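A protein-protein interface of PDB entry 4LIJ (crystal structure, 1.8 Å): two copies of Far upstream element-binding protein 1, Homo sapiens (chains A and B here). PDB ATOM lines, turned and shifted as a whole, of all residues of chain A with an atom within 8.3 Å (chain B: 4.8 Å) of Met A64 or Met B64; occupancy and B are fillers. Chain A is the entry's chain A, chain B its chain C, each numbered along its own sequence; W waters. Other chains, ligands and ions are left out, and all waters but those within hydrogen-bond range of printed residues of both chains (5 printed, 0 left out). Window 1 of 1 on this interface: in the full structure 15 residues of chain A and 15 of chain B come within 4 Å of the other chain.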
ATOM      1  N   MET A  16      -9.635 -10.891   9.121  1.00  0.00           N
ATOM      2  CA  MET A  16     -10.436 -10.864   7.899  1.00  0.00           C
ATOM      3  C   MET A  16     -11.346  -9.664   7.931  1.00  0.00           C
ATOM      4  O   MET A  16     -11.496  -9.007   8.961  1.00  0.00           O
ATOM      5  CB  MET A  16     -11.219 -12.157   7.725  1.00  0.00           C
ATOM      6  CG  MET A  16     -12.033 -12.519   8.922  1.00  0.00           C
ATOM      7  SD  MET A  16     -13.790 -11.680   8.786  1.00  0.00           S
ATOM      8  CE  MET A  16     -14.822 -12.990   9.782  1.00  0.00           C
ATOM      9  N   THR A  17     -11.939  -9.356   6.782  1.00  0.00           N
ATOM     10  CA  THR A  17     -12.813  -8.214   6.655  1.00  0.00           C
ATOM     11  C   THR A  17     -14.214  -8.682   6.251  1.00  0.00           C
ATOM     12  O   THR A  17     -14.350  -9.465   5.333  1.00  0.00           O
ATOM     13  CB  THR A  17     -12.229  -7.199   5.648  1.00  0.00           C
ATOM     14  OG1 THR A  17     -10.986  -6.689   6.156  1.00  0.00           O
ATOM     15  CG2 THR A  17     -13.179  -6.033   5.435  1.00  0.00           C
ATOM     16  N   GLU A  18     -15.222  -8.182   6.960  1.00  0.00           N
ATOM     17  CA  GLU A  18     -16.627  -8.470   6.688  1.00  0.00           C
ATOM     18  C   GLU A  18     -17.429  -7.193   6.503  1.00  0.00           C
ATOM     19  O   GLU A  18     -17.153  -6.200   7.167  1.00  0.00           O
ATOM     20  CB  GLU A  18     -17.233  -9.248   7.849  1.00  0.00           C
ATOM     21  CG  GLU A  18     -17.309 -10.732   7.594  1.00  0.00           C
ATOM     22  CD  GLU A  18     -18.156 -11.442   8.594  1.00  0.00           C
ATOM     23  OE1 GLU A  18     -19.209 -10.896   8.909  1.00  0.00           O
ATOM     24  OE2 GLU A  18     -17.785 -12.536   9.035  1.00  0.00           O
ATOM     25  N   GLU A  19     -18.371  -7.217   5.560  1.00  0.00           N
ATOM     26  CA  GLU A  19     -19.406  -6.182   5.456  1.00  0.00           C
ATOM     27  C   GLU A  19     -20.423  -6.411   6.552  1.00  0.00           C
ATOM     28  O   GLU A  19     -20.660  -7.538   6.952  1.00  0.00           O
ATOM     29  CB  GLU A  19     -20.110  -6.222   4.088  1.00  0.00           C
ATOM     30  CG  GLU A  19     -19.474  -5.343   3.013  1.00  0.00           C
ATOM     31  CD  GLU A  19     -19.824  -3.860   3.134  1.00  0.00           C
ATOM     32  OE1 GLU A  19     -20.913  -3.524   3.646  1.00  0.00           O
ATOM     33  OE2 GLU A  19     -19.009  -3.018   2.696  1.00  0.00           O
ATOM     34  N   TYR A  20     -21.028  -5.330   7.026  1.00  0.00           N
ATOM     35  CA  TYR A  20     -22.078  -5.399   8.002  1.00  0.00           C
ATOM     36  C   TYR A  20     -22.978  -4.166   7.836  1.00  0.00           C
ATOM     37  O   TYR A  20     -22.595  -3.230   7.128  1.00  0.00           O
ATOM     38  CB  TYR A  20     -21.469  -5.461   9.376  1.00  0.00           C
ATOM     39  CG  TYR A  20     -22.448  -5.775  10.441  1.00  0.00           C
ATOM     40  CD1 TYR A  20     -23.198  -6.961  10.405  1.00  0.00           C
ATOM     41  CD2 TYR A  20     -22.647  -4.906  11.480  1.00  0.00           C
ATOM     42  CE1 TYR A  20     -24.112  -7.253  11.396  1.00  0.00           C
ATOM     43  CE2 TYR A  20     -23.554  -5.195  12.478  1.00  0.00           C
ATOM     44  CZ  TYR A  20     -24.278  -6.360  12.437  1.00  0.00           C
ATOM     45  OH  TYR A  20     -25.185  -6.645  13.424  1.00  0.00           O
ATOM     46  N   LYS A  21     -24.180  -4.207   8.410  1.00  0.00           N
ATOM     47  CA  LYS A  21     -25.170  -3.133   8.230  1.00  0.00           C
ATOM     48  C   LYS A  21     -25.690  -2.663   9.565  1.00  0.00           C
ATOM     49  O   LYS A  21     -25.919  -3.487  10.467  1.00  0.00           O
ATOM     50  CB  LYS A  21     -26.374  -3.599   7.412  1.00  0.00           C
ATOM     51  CG  LYS A  21     -26.045  -4.108   6.023  1.00  0.00           C
ATOM     52  CD  LYS A  21     -25.686  -2.988   5.063  1.00  0.00           C
ATOM     53  CE  LYS A  21     -25.119  -3.532   3.754  1.00  0.00           C
ATOM     54  NZ  LYS A  21     -26.071  -4.396   3.006  1.00  0.00           N
ATOM     55  N   ILE A  38     -17.890   4.653  19.292  1.00  0.00           N
ATOM     56  CA  ILE A  38     -17.246   3.755  18.323  1.00  0.00           C
ATOM     57  C   ILE A  38     -15.825   3.390  18.770  1.00  0.00           C
ATOM     58  O   ILE A  38     -15.377   2.254  18.572  1.00  0.00           O
ATOM     59  CB  ILE A  38     -17.318   4.286  16.848  1.00  0.00           C
ATOM     60  CG1 ILE A  38     -16.927   3.205  15.846  1.00  0.00           C
ATOM     61  CG2 ILE A  38     -16.467   5.528  16.621  1.00  0.00           C
ATOM     62  CD1 ILE A  38     -17.872   2.030  15.865  1.00  0.00           C
ATOM     63  N   GLN A  42     -14.750  -0.602  19.282  1.00  0.00           N
ATOM     64  CA  GLN A  42     -13.556  -1.126  18.622  1.00  0.00           C
ATOM     65  C   GLN A  42     -12.585  -1.721  19.641  1.00  0.00           C
ATOM     66  O   GLN A  42     -12.025  -2.805  19.429  1.00  0.00           O
ATOM     67  CB  GLN A  42     -12.883  -0.037  17.785  1.00  0.00           C
ATOM     68  CG  GLN A  42     -13.701   0.323  16.545  1.00  0.00           C
ATOM     69  CD  GLN A  42     -13.090   1.437  15.716  1.00  0.00           C
ATOM     70  OE1 GLN A  42     -12.620   1.219  14.589  1.00  0.00           O
ATOM     71  NE2 GLN A  42     -13.130   2.653  16.255  1.00  0.00           N
ATOM     72  N   CYS A  47     -11.794  -5.068  16.973  1.00  0.00           N
ATOM     73  CA  CYS A  47     -12.163  -4.946  15.581  1.00  0.00           C
ATOM     74  C   CYS A  47     -12.030  -3.476  15.095  1.00  0.00           C
ATOM     75  O   CYS A  47     -12.420  -2.569  15.809  1.00  0.00           O
ATOM     76  CB  CYS A  47     -13.611  -5.495  15.447  1.00  0.00           C
ATOM     77  SG  CYS A  47     -14.198  -5.771  13.798  1.00  0.00           S
ATOM     78  N   LYS A  48     -11.501  -3.246  13.896  1.00  0.00           N
ATOM     79  CA  LYS A  48     -11.639  -1.947  13.214  1.00  0.00           C
ATOM     80  C   LYS A  48     -13.034  -1.869  12.590  1.00  0.00           C
ATOM     81  O   LYS A  48     -13.467  -2.787  11.899  1.00  0.00           O
ATOM     82  CB  LYS A  48     -10.600  -1.779  12.110  1.00  0.00           C
ATOM     83  CG  LYS A  48     -10.708  -0.471  11.323  1.00  0.00           C
ATOM     84  CD  LYS A  48     -10.192   0.705  12.114  1.00  0.00           C
ATOM     85  CE  LYS A  48     -10.212   1.953  11.244  1.00  0.00           C
ATOM     86  NZ  LYS A  48      -9.585   3.101  11.933  1.00  0.00           N
ATOM     87  N   ILE A  49     -13.752  -0.783  12.853  1.00  0.00           N
ATOM     88  CA  ILE A  49     -15.126  -0.608  12.350  1.00  0.00           C
ATOM     89  C   ILE A  49     -15.167   0.687  11.550  1.00  0.00           C
ATOM     90  O   ILE A  49     -15.059   1.773  12.127  1.00  0.00           O
ATOM     91  CB  ILE A  49     -16.163  -0.549  13.494  1.00  0.00           C
ATOM     92  CG1 ILE A  49     -16.082  -1.817  14.372  1.00  0.00           C
ATOM     93  CG2 ILE A  49     -17.583  -0.392  12.934  1.00  0.00           C
ATOM     94  CD1 ILE A  49     -16.889  -1.761  15.650  1.00  0.00           C
ATOM     95  N   GLN A  50     -15.349   0.553  10.239  1.00  0.00           N
ATOM     96  CA  GLN A  50     -15.445   1.685   9.334  1.00  0.00           C
ATOM     97  C   GLN A  50     -16.869   1.789   8.822  1.00  0.00           C
ATOM     98  O   GLN A  50     -17.471   0.791   8.411  1.00  0.00           O
ATOM     99  CB  GLN A  50     -14.454   1.501   8.188  1.00  0.00           C
ATOM    100  CG  GLN A  50     -13.011   1.532   8.680  1.00  0.00           C
ATOM    101  CD  GLN A  50     -12.016   1.026   7.654  1.00  0.00           C
ATOM    102  OE1 GLN A  50     -11.780  -0.183   7.532  1.00  0.00           O
ATOM    103  NE2 GLN A  50     -11.389   1.947   6.948  1.00  0.00           N
ATOM    104  N   ILE A  51     -17.430   2.992   8.886  1.00  0.00           N
ATOM    105  CA  ILE A  51     -18.848   3.203   8.529  1.00  0.00           C
ATOM    106  C   ILE A  51     -18.935   4.124   7.314  1.00  0.00           C
ATOM    107  O   ILE A  51     -18.244   5.136   7.260  1.00  0.00           O
ATOM    108  CB  ILE A  51     -19.601   3.814   9.710  1.00  0.00           C
ATOM    109  CG1 ILE A  51     -19.394   2.918  10.941  1.00  0.00           C
ATOM    110  CG2 ILE A  51     -21.082   3.987   9.386  1.00  0.00           C
ATOM    111  CD1 ILE A  51     -19.970   3.486  12.217  1.00  0.00           C
ATOM    112  N   ALA A  52     -19.738   3.736   6.330  1.00  0.00           N
ATOM    113  CA  ALA A  52     -19.911   4.553   5.125  1.00  0.00           C
ATOM    114  C   ALA A  52     -20.581   5.873   5.508  1.00  0.00           C
ATOM    115  O   ALA A  52     -21.308   5.941   6.507  1.00  0.00           O
ATOM    116  CB  ALA A  52     -20.736   3.804   4.080  1.00  0.00           C
ATOM    117  N   PRO A  53     -20.342   6.932   4.729  1.00  0.00           N
ATOM    118  CA  PRO A  53     -20.823   8.273   5.121  1.00  0.00           C
ATOM    119  C   PRO A  53     -22.270   8.620   4.767  1.00  0.00           C
ATOM    120  O   PRO A  53     -22.746   9.688   5.157  1.00  0.00           O
ATOM    121  CB  PRO A  53     -19.865   9.194   4.363  1.00  0.00           C
ATOM    122  CG  PRO A  53     -19.573   8.436   3.115  1.00  0.00           C
ATOM    123  CD  PRO A  53     -19.411   7.006   3.596  1.00  0.00           C
ATOM    124  N   ARG A  61     -27.030   1.465   6.710  1.00  0.00           N
ATOM    125  CA  ARG A  61     -25.734   2.055   6.379  1.00  0.00           C
ATOM    126  C   ARG A  61     -24.700   0.934   6.421  1.00  0.00           C
ATOM    127  O   ARG A  61     -24.665   0.153   7.370  1.00  0.00           O
ATOM    128  CB  ARG A  61     -25.365   3.118   7.407  1.00  0.00           C
ATOM    129  CG  ARG A  61     -24.103   3.913   7.073  1.00  0.00           C
ATOM    130  CD  ARG A  61     -24.380   4.976   6.011  1.00  0.00           C
ATOM    131  NE  ARG A  61     -25.253   6.022   6.544  1.00  0.00           N
ATOM    132  CZ  ARG A  61     -24.856   7.088   7.241  1.00  0.00           C
ATOM    133  NH1 ARG A  61     -23.581   7.296   7.517  1.00  0.00           N
ATOM    134  NH2 ARG A  61     -25.768   7.971   7.667  1.00  0.00           N
ATOM    135  N   SER A  62     -23.902   0.819   5.379  1.00  0.00           N
ATOM    136  CA  SER A  62     -22.851  -0.212   5.320  1.00  0.00           C
ATOM    137  C   SER A  62     -21.657   0.108   6.210  1.00  0.00           C
ATOM    138  O   SER A  62     -21.220   1.252   6.265  1.00  0.00           O
ATOM    139  CB  SER A  62     -22.335  -0.387   3.893  1.00  0.00           C
ATOM    140  OG  SER A  62     -23.362  -0.827   3.037  1.00  0.00           O
ATOM    141  N   CYS A  63     -21.136  -0.949   6.843  1.00  0.00           N
ATOM    142  CA  CYS A  63     -19.944  -0.909   7.668  1.00  0.00           C
ATOM    143  C   CYS A  63     -18.983  -1.994   7.200  1.00  0.00           C
ATOM    144  O   CYS A  63     -19.419  -2.997   6.617  1.00  0.00           O
ATOM    145  CB  CYS A  63     -20.297  -1.206   9.120  1.00  0.00           C
ATOM    146  SG  CYS A  63     -21.581  -0.132   9.806  1.00  0.00           S
ATOM    147  N   MET A  64     -17.687  -1.760   7.402  1.00  0.00           N
ATOM    148  CA  MET A  64     -16.671  -2.753   7.151  1.00  0.00           C
ATOM    149  C   MET A  64     -16.011  -3.055   8.475  1.00  0.00           C
ATOM    150  O   MET A  64     -15.512  -2.144   9.156  1.00  0.00           O
ATOM    151  CB  MET A  64     -15.703  -2.173   6.131  1.00  0.00           C
ATOM    152  CG  MET A  64     -14.705  -3.168   5.584  1.00  0.00           C
ATOM    153  SD  MET A  64     -13.924  -2.455   3.906  1.00  0.00           S
ATOM    154  CE  MET A  64     -13.294  -0.719   4.559  1.00  0.00           C
ATOM    155  N   LEU A  65     -15.983  -4.335   8.833  1.00  0.00           N
ATOM    156  CA  LEU A  65     -15.370  -4.805  10.067  1.00  0.00           C
ATOM    157  C   LEU A  65     -14.128  -5.611   9.768  1.00  0.00           C
ATOM    158  O   LEU A  65     -14.174  -6.521   8.943  1.00  0.00           O
ATOM    159  CB  LEU A  65     -16.341  -5.701  10.813  1.00  0.00           C
ATOM    160  CG  LEU A  65     -17.769  -5.215  10.948  1.00  0.00           C
ATOM    161  CD1 LEU A  65     -18.552  -6.299  11.619  1.00  0.00           C
ATOM    162  CD2 LEU A  65     -17.719  -3.917  11.690  1.00  0.00           C
ATOM    163  N   THR A  66     -13.019  -5.265  10.423  1.00  0.00           N
ATOM    164  CA  THR A  66     -11.752  -5.959  10.188  1.00  0.00           C
ATOM    165  C   THR A  66     -11.149  -6.426  11.506  1.00  0.00           C
ATOM    166  O   THR A  66     -10.879  -5.635  12.402  1.00  0.00           O
ATOM    167  CB  THR A  66     -10.716  -5.080   9.451  1.00  0.00           C
ATOM    168  OG1 THR A  66     -11.242  -4.676   8.183  1.00  0.00           O
ATOM    169  CG2 THR A  66      -9.415  -5.875   9.221  1.00  0.00           C
ATOM    170  N   GLY A  67     -10.940  -7.730  11.597  1.00  0.00           N
ATOM    171  CA  GLY A  67     -10.406  -8.360  12.788  1.00  0.00           C
ATOM    172  C   GLY A  67     -10.372  -9.858  12.606  1.00  0.00           C
ATOM    173  O   GLY A  67     -10.829 -10.377  11.584  1.00  0.00           O
ATOM    174  N   VAL A  72     -14.646  -9.996  15.023  1.00  0.00           N
ATOM    175  CA  VAL A  72     -15.721  -9.549  14.136  1.00  0.00           C
ATOM    176  C   VAL A  72     -17.089  -9.920  14.723  1.00  0.00           C
ATOM    177  O   VAL A  72     -18.004  -9.092  14.767  1.00  0.00           O
ATOM    178  CB  VAL A  72     -15.542 -10.128  12.725  1.00  0.00           C
ATOM    179  CG1 VAL A  72     -16.820  -9.980  11.896  1.00  0.00           C
ATOM    180  CG2 VAL A  72     -14.353  -9.457  12.056  1.00  0.00           C
ATOM    181  N   ALA A  75     -17.793  -7.644  17.640  1.00  0.00           N
ATOM    182  CA  ALA A  75     -18.182  -6.305  17.195  1.00  0.00           C
ATOM    183  C   ALA A  75     -19.661  -6.270  16.780  1.00  0.00           C
ATOM    184  O   ALA A  75     -20.385  -5.354  17.172  1.00  0.00           O
ATOM    185  CB  ALA A  75     -17.300  -5.831  16.069  1.00  0.00           C
ATOM    186  N   LEU A  79     -22.348  -3.781  18.528  1.00  0.00           N
ATOM    187  CA  LEU A  79     -23.127  -2.877  17.697  1.00  0.00           C
ATOM    188  C   LEU A  79     -24.629  -3.118  17.907  1.00  0.00           C
ATOM    189  O   LEU A  79     -25.403  -2.157  18.062  1.00  0.00           O
ATOM    190  CB  LEU A  79     -22.779  -3.067  16.222  1.00  0.00           C
ATOM    191  CG  LEU A  79     -21.415  -2.484  15.848  1.00  0.00           C
ATOM    192  CD1 LEU A  79     -20.993  -3.006  14.485  1.00  0.00           C
ATOM    193  CD2 LEU A  79     -21.464  -0.960  15.832  1.00  0.00           C
ATOM    194  N   THR B  17     -23.435   2.138  -1.737  1.00  0.00           N
ATOM    195  CA  THR B  17     -22.162   1.639  -1.225  1.00  0.00           C
ATOM    196  C   THR B  17     -21.857   0.274  -1.845  1.00  0.00           C
ATOM    197  O   THR B  17     -22.721  -0.583  -1.911  1.00  0.00           O
ATOM    198  CB  THR B  17     -22.178   1.561   0.318  1.00  0.00           C
ATOM    199  OG1 THR B  17     -22.327   2.882   0.855  1.00  0.00           O
ATOM    200  CG2 THR B  17     -20.890   0.961   0.855  1.00  0.00           C
ATOM    201  N   GLU B  18     -20.624   0.111  -2.321  1.00  0.00           N
ATOM    202  CA  GLU B  18     -20.131  -1.127  -2.902  1.00  0.00           C
ATOM    203  C   GLU B  18     -18.840  -1.563  -2.203  1.00  0.00           C
ATOM    204  O   GLU B  18     -18.000  -0.718  -1.890  1.00  0.00           O
ATOM    205  CB  GLU B  18     -19.821  -0.902  -4.396  1.00  0.00           C
ATOM    206  CG  GLU B  18     -20.870  -1.358  -5.368  1.00  0.00           C
ATOM    207  CD  GLU B  18     -20.359  -1.239  -6.797  1.00  0.00           C
ATOM    208  OE1 GLU B  18     -19.152  -1.487  -7.027  1.00  0.00           O
ATOM    209  OE2 GLU B  18     -21.151  -0.871  -7.689  1.00  0.00           O
ATOM    210  N   GLU B  19     -18.685  -2.874  -1.985  1.00  0.00           N
ATOM    211  CA  GLU B  19     -17.379  -3.466  -1.672  1.00  0.00           C
ATOM    212  C   GLU B  19     -16.540  -3.476  -2.934  1.00  0.00           C
ATOM    213  O   GLU B  19     -17.052  -3.608  -4.035  1.00  0.00           O
ATOM    214  CB  GLU B  19     -17.501  -4.903  -1.147  1.00  0.00           C
ATOM    215  CG  GLU B  19     -17.633  -5.018   0.364  1.00  0.00           C
ATOM    216  CD  GLU B  19     -16.305  -4.881   1.123  1.00  0.00           C
ATOM    217  OE1 GLU B  19     -15.236  -5.230   0.571  1.00  0.00           O
ATOM    218  OE2 GLU B  19     -16.333  -4.443   2.295  1.00  0.00           O
ATOM    219  N   LYS B  48     -16.460   8.343  -1.753  1.00  0.00           N
ATOM    220  CA  LYS B  48     -15.731   8.062  -0.523  1.00  0.00           C
ATOM    221  C   LYS B  48     -15.079   6.695  -0.689  1.00  0.00           C
ATOM    222  O   LYS B  48     -15.761   5.746  -1.073  1.00  0.00           O
ATOM    223  CB  LYS B  48     -16.679   8.065   0.656  1.00  0.00           C
ATOM    224  CG  LYS B  48     -16.009   7.766   1.985  1.00  0.00           C
ATOM    225  CD  LYS B  48     -15.237   8.973   2.497  1.00  0.00           C
ATOM    226  CE  LYS B  48     -14.668   8.662   3.867  1.00  0.00           C
ATOM    227  NZ  LYS B  48     -14.044   9.857   4.483  1.00  0.00           N
ATOM    228  N   ILE B  49     -13.778   6.597  -0.423  1.00  0.00           N
ATOM    229  CA  ILE B  49     -13.037   5.345  -0.614  1.00  0.00           C
ATOM    230  C   ILE B  49     -12.392   4.973   0.716  1.00  0.00           C
ATOM    231  O   ILE B  49     -11.475   5.653   1.185  1.00  0.00           O
ATOM    232  CB  ILE B  49     -11.935   5.500  -1.684  1.00  0.00           C
ATOM    233  CG1 ILE B  49     -12.556   5.975  -3.005  1.00  0.00           C
ATOM    234  CG2 ILE B  49     -11.194   4.186  -1.869  1.00  0.00           C
ATOM    235  CD1 ILE B  49     -11.548   6.416  -4.030  1.00  0.00           C
ATOM    236  N   GLN B  50     -12.953   3.965   1.371  1.00  0.00           N
ATOM    237  CA  GLN B  50     -12.503   3.555   2.689  1.00  0.00           C
ATOM    238  C   GLN B  50     -11.785   2.230   2.514  1.00  0.00           C
ATOM    239  O   GLN B  50     -12.302   1.327   1.854  1.00  0.00           O
ATOM    240  CB  GLN B  50     -13.680   3.446   3.658  1.00  0.00           C
ATOM    241  CG  GLN B  50     -14.291   4.816   3.968  1.00  0.00           C
ATOM    242  CD  GLN B  50     -15.641   4.751   4.663  1.00  0.00           C
ATOM    243  OE1 GLN B  50     -16.679   4.545   4.034  1.00  0.00           O
ATOM    244  NE2 GLN B  50     -15.630   4.928   5.965  1.00  0.00           N
ATOM    245  N   ILE B  51     -10.585   2.145   3.040  1.00  0.00           N
ATOM    246  CA  ILE B  51      -9.743   1.008   2.817  1.00  0.00           C
ATOM    247  C   ILE B  51      -9.522   0.327   4.145  1.00  0.00           C
ATOM    248  O   ILE B  51      -9.180   0.980   5.135  1.00  0.00           O
ATOM    249  CB  ILE B  51      -8.397   1.452   2.194  1.00  0.00           C
ATOM    250  CG1 ILE B  51      -8.664   2.253   0.908  1.00  0.00           C
ATOM    251  CG2 ILE B  51      -7.533   0.247   1.887  1.00  0.00           C
ATOM    252  CD1 ILE B  51      -7.420   2.869   0.281  1.00  0.00           C
ATOM    253  N   ALA B  52      -9.709  -0.988   4.165  1.00  0.00           N
ATOM    254  CA  ALA B  52      -9.474  -1.762   5.387  1.00  0.00           C
ATOM    255  C   ALA B  52      -7.976  -1.702   5.737  1.00  0.00           C
ATOM    256  O   ALA B  52      -7.133  -1.517   4.862  1.00  0.00           O
ATOM    257  CB  ALA B  52      -9.933  -3.198   5.203  1.00  0.00           C
ATOM    258  N   SER B  62      -9.715  -5.172   1.097  1.00  0.00           N
ATOM    259  CA  SER B  62     -11.103  -4.735   0.925  1.00  0.00           C
ATOM    260  C   SER B  62     -11.255  -3.246   1.109  1.00  0.00           C
ATOM    261  O   SER B  62     -10.619  -2.635   1.986  1.00  0.00           O
ATOM    262  CB  SER B  62     -12.031  -5.413   1.907  1.00  0.00           C
ATOM    263  OG  SER B  62     -12.048  -6.809   1.685  1.00  0.00           O
ATOM    264  N   CYS B  63     -12.080  -2.676   0.238  1.00  0.00           N
ATOM    265  CA  CYS B  63     -12.401  -1.247   0.229  1.00  0.00           C
ATOM    266  C   CYS B  63     -13.910  -1.148   0.235  1.00  0.00           C
ATOM    267  O   CYS B  63     -14.601  -2.042  -0.265  1.00  0.00           O
ATOM    268  CB  CYS B  63     -11.864  -0.567  -1.041  1.00  0.00           C
ATOM    269  SG  CYS B  63     -10.085  -0.759  -1.257  1.00  0.00           S
ATOM    270  N   MET B  64     -14.417  -0.047   0.747  1.00  0.00           N
ATOM    271  CA  MET B  64     -15.821   0.304   0.607  1.00  0.00           C
ATOM    272  C   MET B  64     -15.865   1.601  -0.170  1.00  0.00           C
ATOM    273  O   MET B  64     -15.223   2.584   0.204  1.00  0.00           O
ATOM    274  CB  MET B  64     -16.389   0.406   2.025  1.00  0.00           C
ATOM    275  CG  MET B  64     -17.889   0.552   2.110  1.00  0.00           C
ATOM    276  SD  MET B  64     -18.506   0.132   3.953  1.00  0.00           S
ATOM    277  CE  MET B  64     -17.344   1.368   4.946  1.00  0.00           C
ATOM    278  N   LEU B  65     -16.644   1.607  -1.256  1.00  0.00           N
ATOM    279  CA  LEU B  65     -16.836   2.776  -2.093  1.00  0.00           C
ATOM    280  C   LEU B  65     -18.257   3.275  -1.914  1.00  0.00           C
ATOM    281  O   LEU B  65     -19.218   2.512  -2.058  1.00  0.00           O
ATOM    282  CB  LEU B  65     -16.644   2.453  -3.578  1.00  0.00           C
ATOM    283  CG  LEU B  65     -15.353   1.760  -3.982  1.00  0.00           C
ATOM    284  CD1 LEU B  65     -15.346   1.557  -5.508  1.00  0.00           C
ATOM    285  CD2 LEU B  65     -14.138   2.538  -3.526  1.00  0.00           C
ATOM    286  N   THR B  66     -18.403   4.555  -1.619  1.00  0.00           N
ATOM    287  CA  THR B  66     -19.734   5.159  -1.458  1.00  0.00           C
ATOM    288  C   THR B  66     -19.879   6.373  -2.364  1.00  0.00           C
ATOM    289  O   THR B  66     -19.087   7.319  -2.285  1.00  0.00           O
ATOM    290  CB  THR B  66     -20.011   5.583  -0.007  1.00  0.00           C
ATOM    291  OG1 THR B  66     -19.926   4.439   0.849  1.00  0.00           O
ATOM    292  CG2 THR B  66     -21.408   6.204   0.130  1.00  0.00           C
HETATM  293  O   HOH W   1      -8.862  -6.426   3.703  1.00  0.00           O
HETATM  294  O   HOH W   2     -24.108   2.633   3.322  1.00  0.00           O
HETATM  295  O   HOH W   3     -14.224  -8.292   2.458  1.00  0.00           O
HETATM  296  O   HOH W   4     -22.561  -2.536   0.806  1.00  0.00           O
HETATM  297  O   HOH W   5      -8.193   1.326   7.777  1.00  0.00           O
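The side-chain amide nitrogen of Gln A50 is in hydrogen-bond range of the backbone carbonyl oxygen of Ile B51 (3.0 Å). The side-chain amide nitrogen (NE2) of Gln B50 is in hydrogen-bond range of the backbone carbonyl oxygen (O) of Ile A51 (2.9 Å). OE2 of Glu B19 sits close to OE2 of Glu A19. The side-chain sulfur (SD) of Met B64 sits close to the side-chain carboxylate (OE2) of Glu A19, 3.4 Å away. The side-chain sulfur (SD) of Met B64 sits close to the backbone carbonyl oxygen (O) of Ser A62 (3.7 Å). The side-chain carboxylate of Glu B19 sits close to the side-chain sulfur of Met A64, at 3.5 Å.
N of Cys A63 lies within hydrogen-bond range of O of Tyr A20 (2.7 Å). The backbone carbonyl oxygen of Thr A66 is in hydrogen-bond range of the backbone NH of Lys A48, at 2.9 Å. The backbone NH (N) of Met A64 sits at hydrogen-bond distance from the backbone carbonyl oxygen (O) of Gln A50 (2.8 Å). The backbone carbonyl oxygen (O) of Ser A62 lies within hydrogen-bond range of the backbone NH (N) of Ala A52 (2.9 Å). The backbone carbonyl oxygen of Gln B50 sits at hydrogen-bond distance from the backbone NH of Met B64 (2.8 Å). The backbone carbonyl oxygen (O) of Ser B62 sits at hydrogen-bond distance from the backbone NH (N) of Ala B52, at 2.9 Å.
Among the printed residues, merely in contact across the chains: Thr A17 with Ala B52 (3.8 Å), Thr A17 with Ser B62 (3.8 Å), Gln A50 with Ala B52 (3.5 Å), Gln A50 with Met B64 (3.5 Å), Ile A51 with Met B64 (3.97 Å), Ala A52 with Thr B17 (3.7 Å), Ala A52 with Gln B50 (3.4 Å), Ala A52 with Met B64 (3.6 Å), Ala A52 with Thr B66 (3.4 Å), Pro A53 with Lys B48 (3.8 Å), Pro A53 with Gln B50 (3.7 Å), Pro A53 with Thr B66 (3.8 Å), Ser A62 with Thr B17 (3.6 Å), Cys A63 with Met B64 (3.9 Å), Met A64 with Gln B50 (3.5 Å), Met A64 with Ile B51 (3.9 Å), Met A64 with Ala B52 (3.6 Å), Met A64 with Ser B62 (3.8 Å), Met A64 with Cys B63 (3.9 Å), Met A64 with Met B64 (3.99 Å) and Thr A66 with Ala B52 (3.6 Å).
Of the printed residues of chain B, Gln A50 touches Ile B51, Ala B52 and Met B64. Of the printed residues of chain B, Pro A53 touches Lys B48 (3.8 Å), Gln B50 (3.7 Å) and Thr B66 (3.8 Å). Arg A61 touches none of the printed residues of chain B. Of the printed residues of chain B, Met A64 touches Glu B19, Gln B50, Ile B51, Ala B52, Ser B62, Cys B63 and Met B64. Of the printed residues of chain A, Lys B48 touches Pro A53 (3.8 Å). Printed residues of chain A within 4 Å of Met B64: Glu A19 (3.4 Å), Gln A50 (3.5 Å), Ile A51 (3.97 Å), Ala A52 (3.6 Å), Ser A62 (3.7 Å), Cys A63 (3.9 Å) and Met A64 (3.99 Å).
Printed residues of chain B that touch a printed residue of chain A: Thr B17, Glu B19, Lys B48, Gln B50, Ile B51, Ala B52, Ser B62, Cys B63, Met B64 and Thr B66. Hydrophobic or aromatic side chains of chain B that line the printed part of chain A: Ala B52 and Met B64. Hydrophobic or aromatic side chains of chain A within 4 Å of the printed part of chain B: Ala A52, Pro A53 and Met A64. Among the printed residues, 27 pairs touch across the chains.
Thr A17 touches Ala B52, and with the chains exchanged Ala A52 touches Thr B17. Glu B19 touches its own counterpart, Glu A19. Gln A50 touches Ile B51, and with the chains exchanged Ile A51 touches Gln B50. Cys A63 touches Met B64, and with the chains exchanged Met A64 touches Cys B63. Of the 27 pairs that touch across the chains among the printed residues, 24 have their exchanged pair printed and touching as well.
Water W3 bridges OG of Ser B62 (2.7 Å) and O of Thr A17 (3.1 Å). Water W2 lies within hydrogen-bond range of N of Ser A62 and OG1 of Thr B17. Water W5 bridges O of Ile B51 (2.8 Å) and NE2 of Gln A50 (3.4 Å). Water W4 lies within hydrogen-bond range of the side-chain hydroxyl of Ser A62 (2.9 Å), the backbone carbonyl oxygen of Thr B17 (3.3 Å) and the side-chain carboxylate of Glu A19 (3.4 Å). Water W1 bridges the backbone NH of Ser B62 (3.0 Å) and the side-chain hydroxyl of Thr A17 (3.3 Å).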
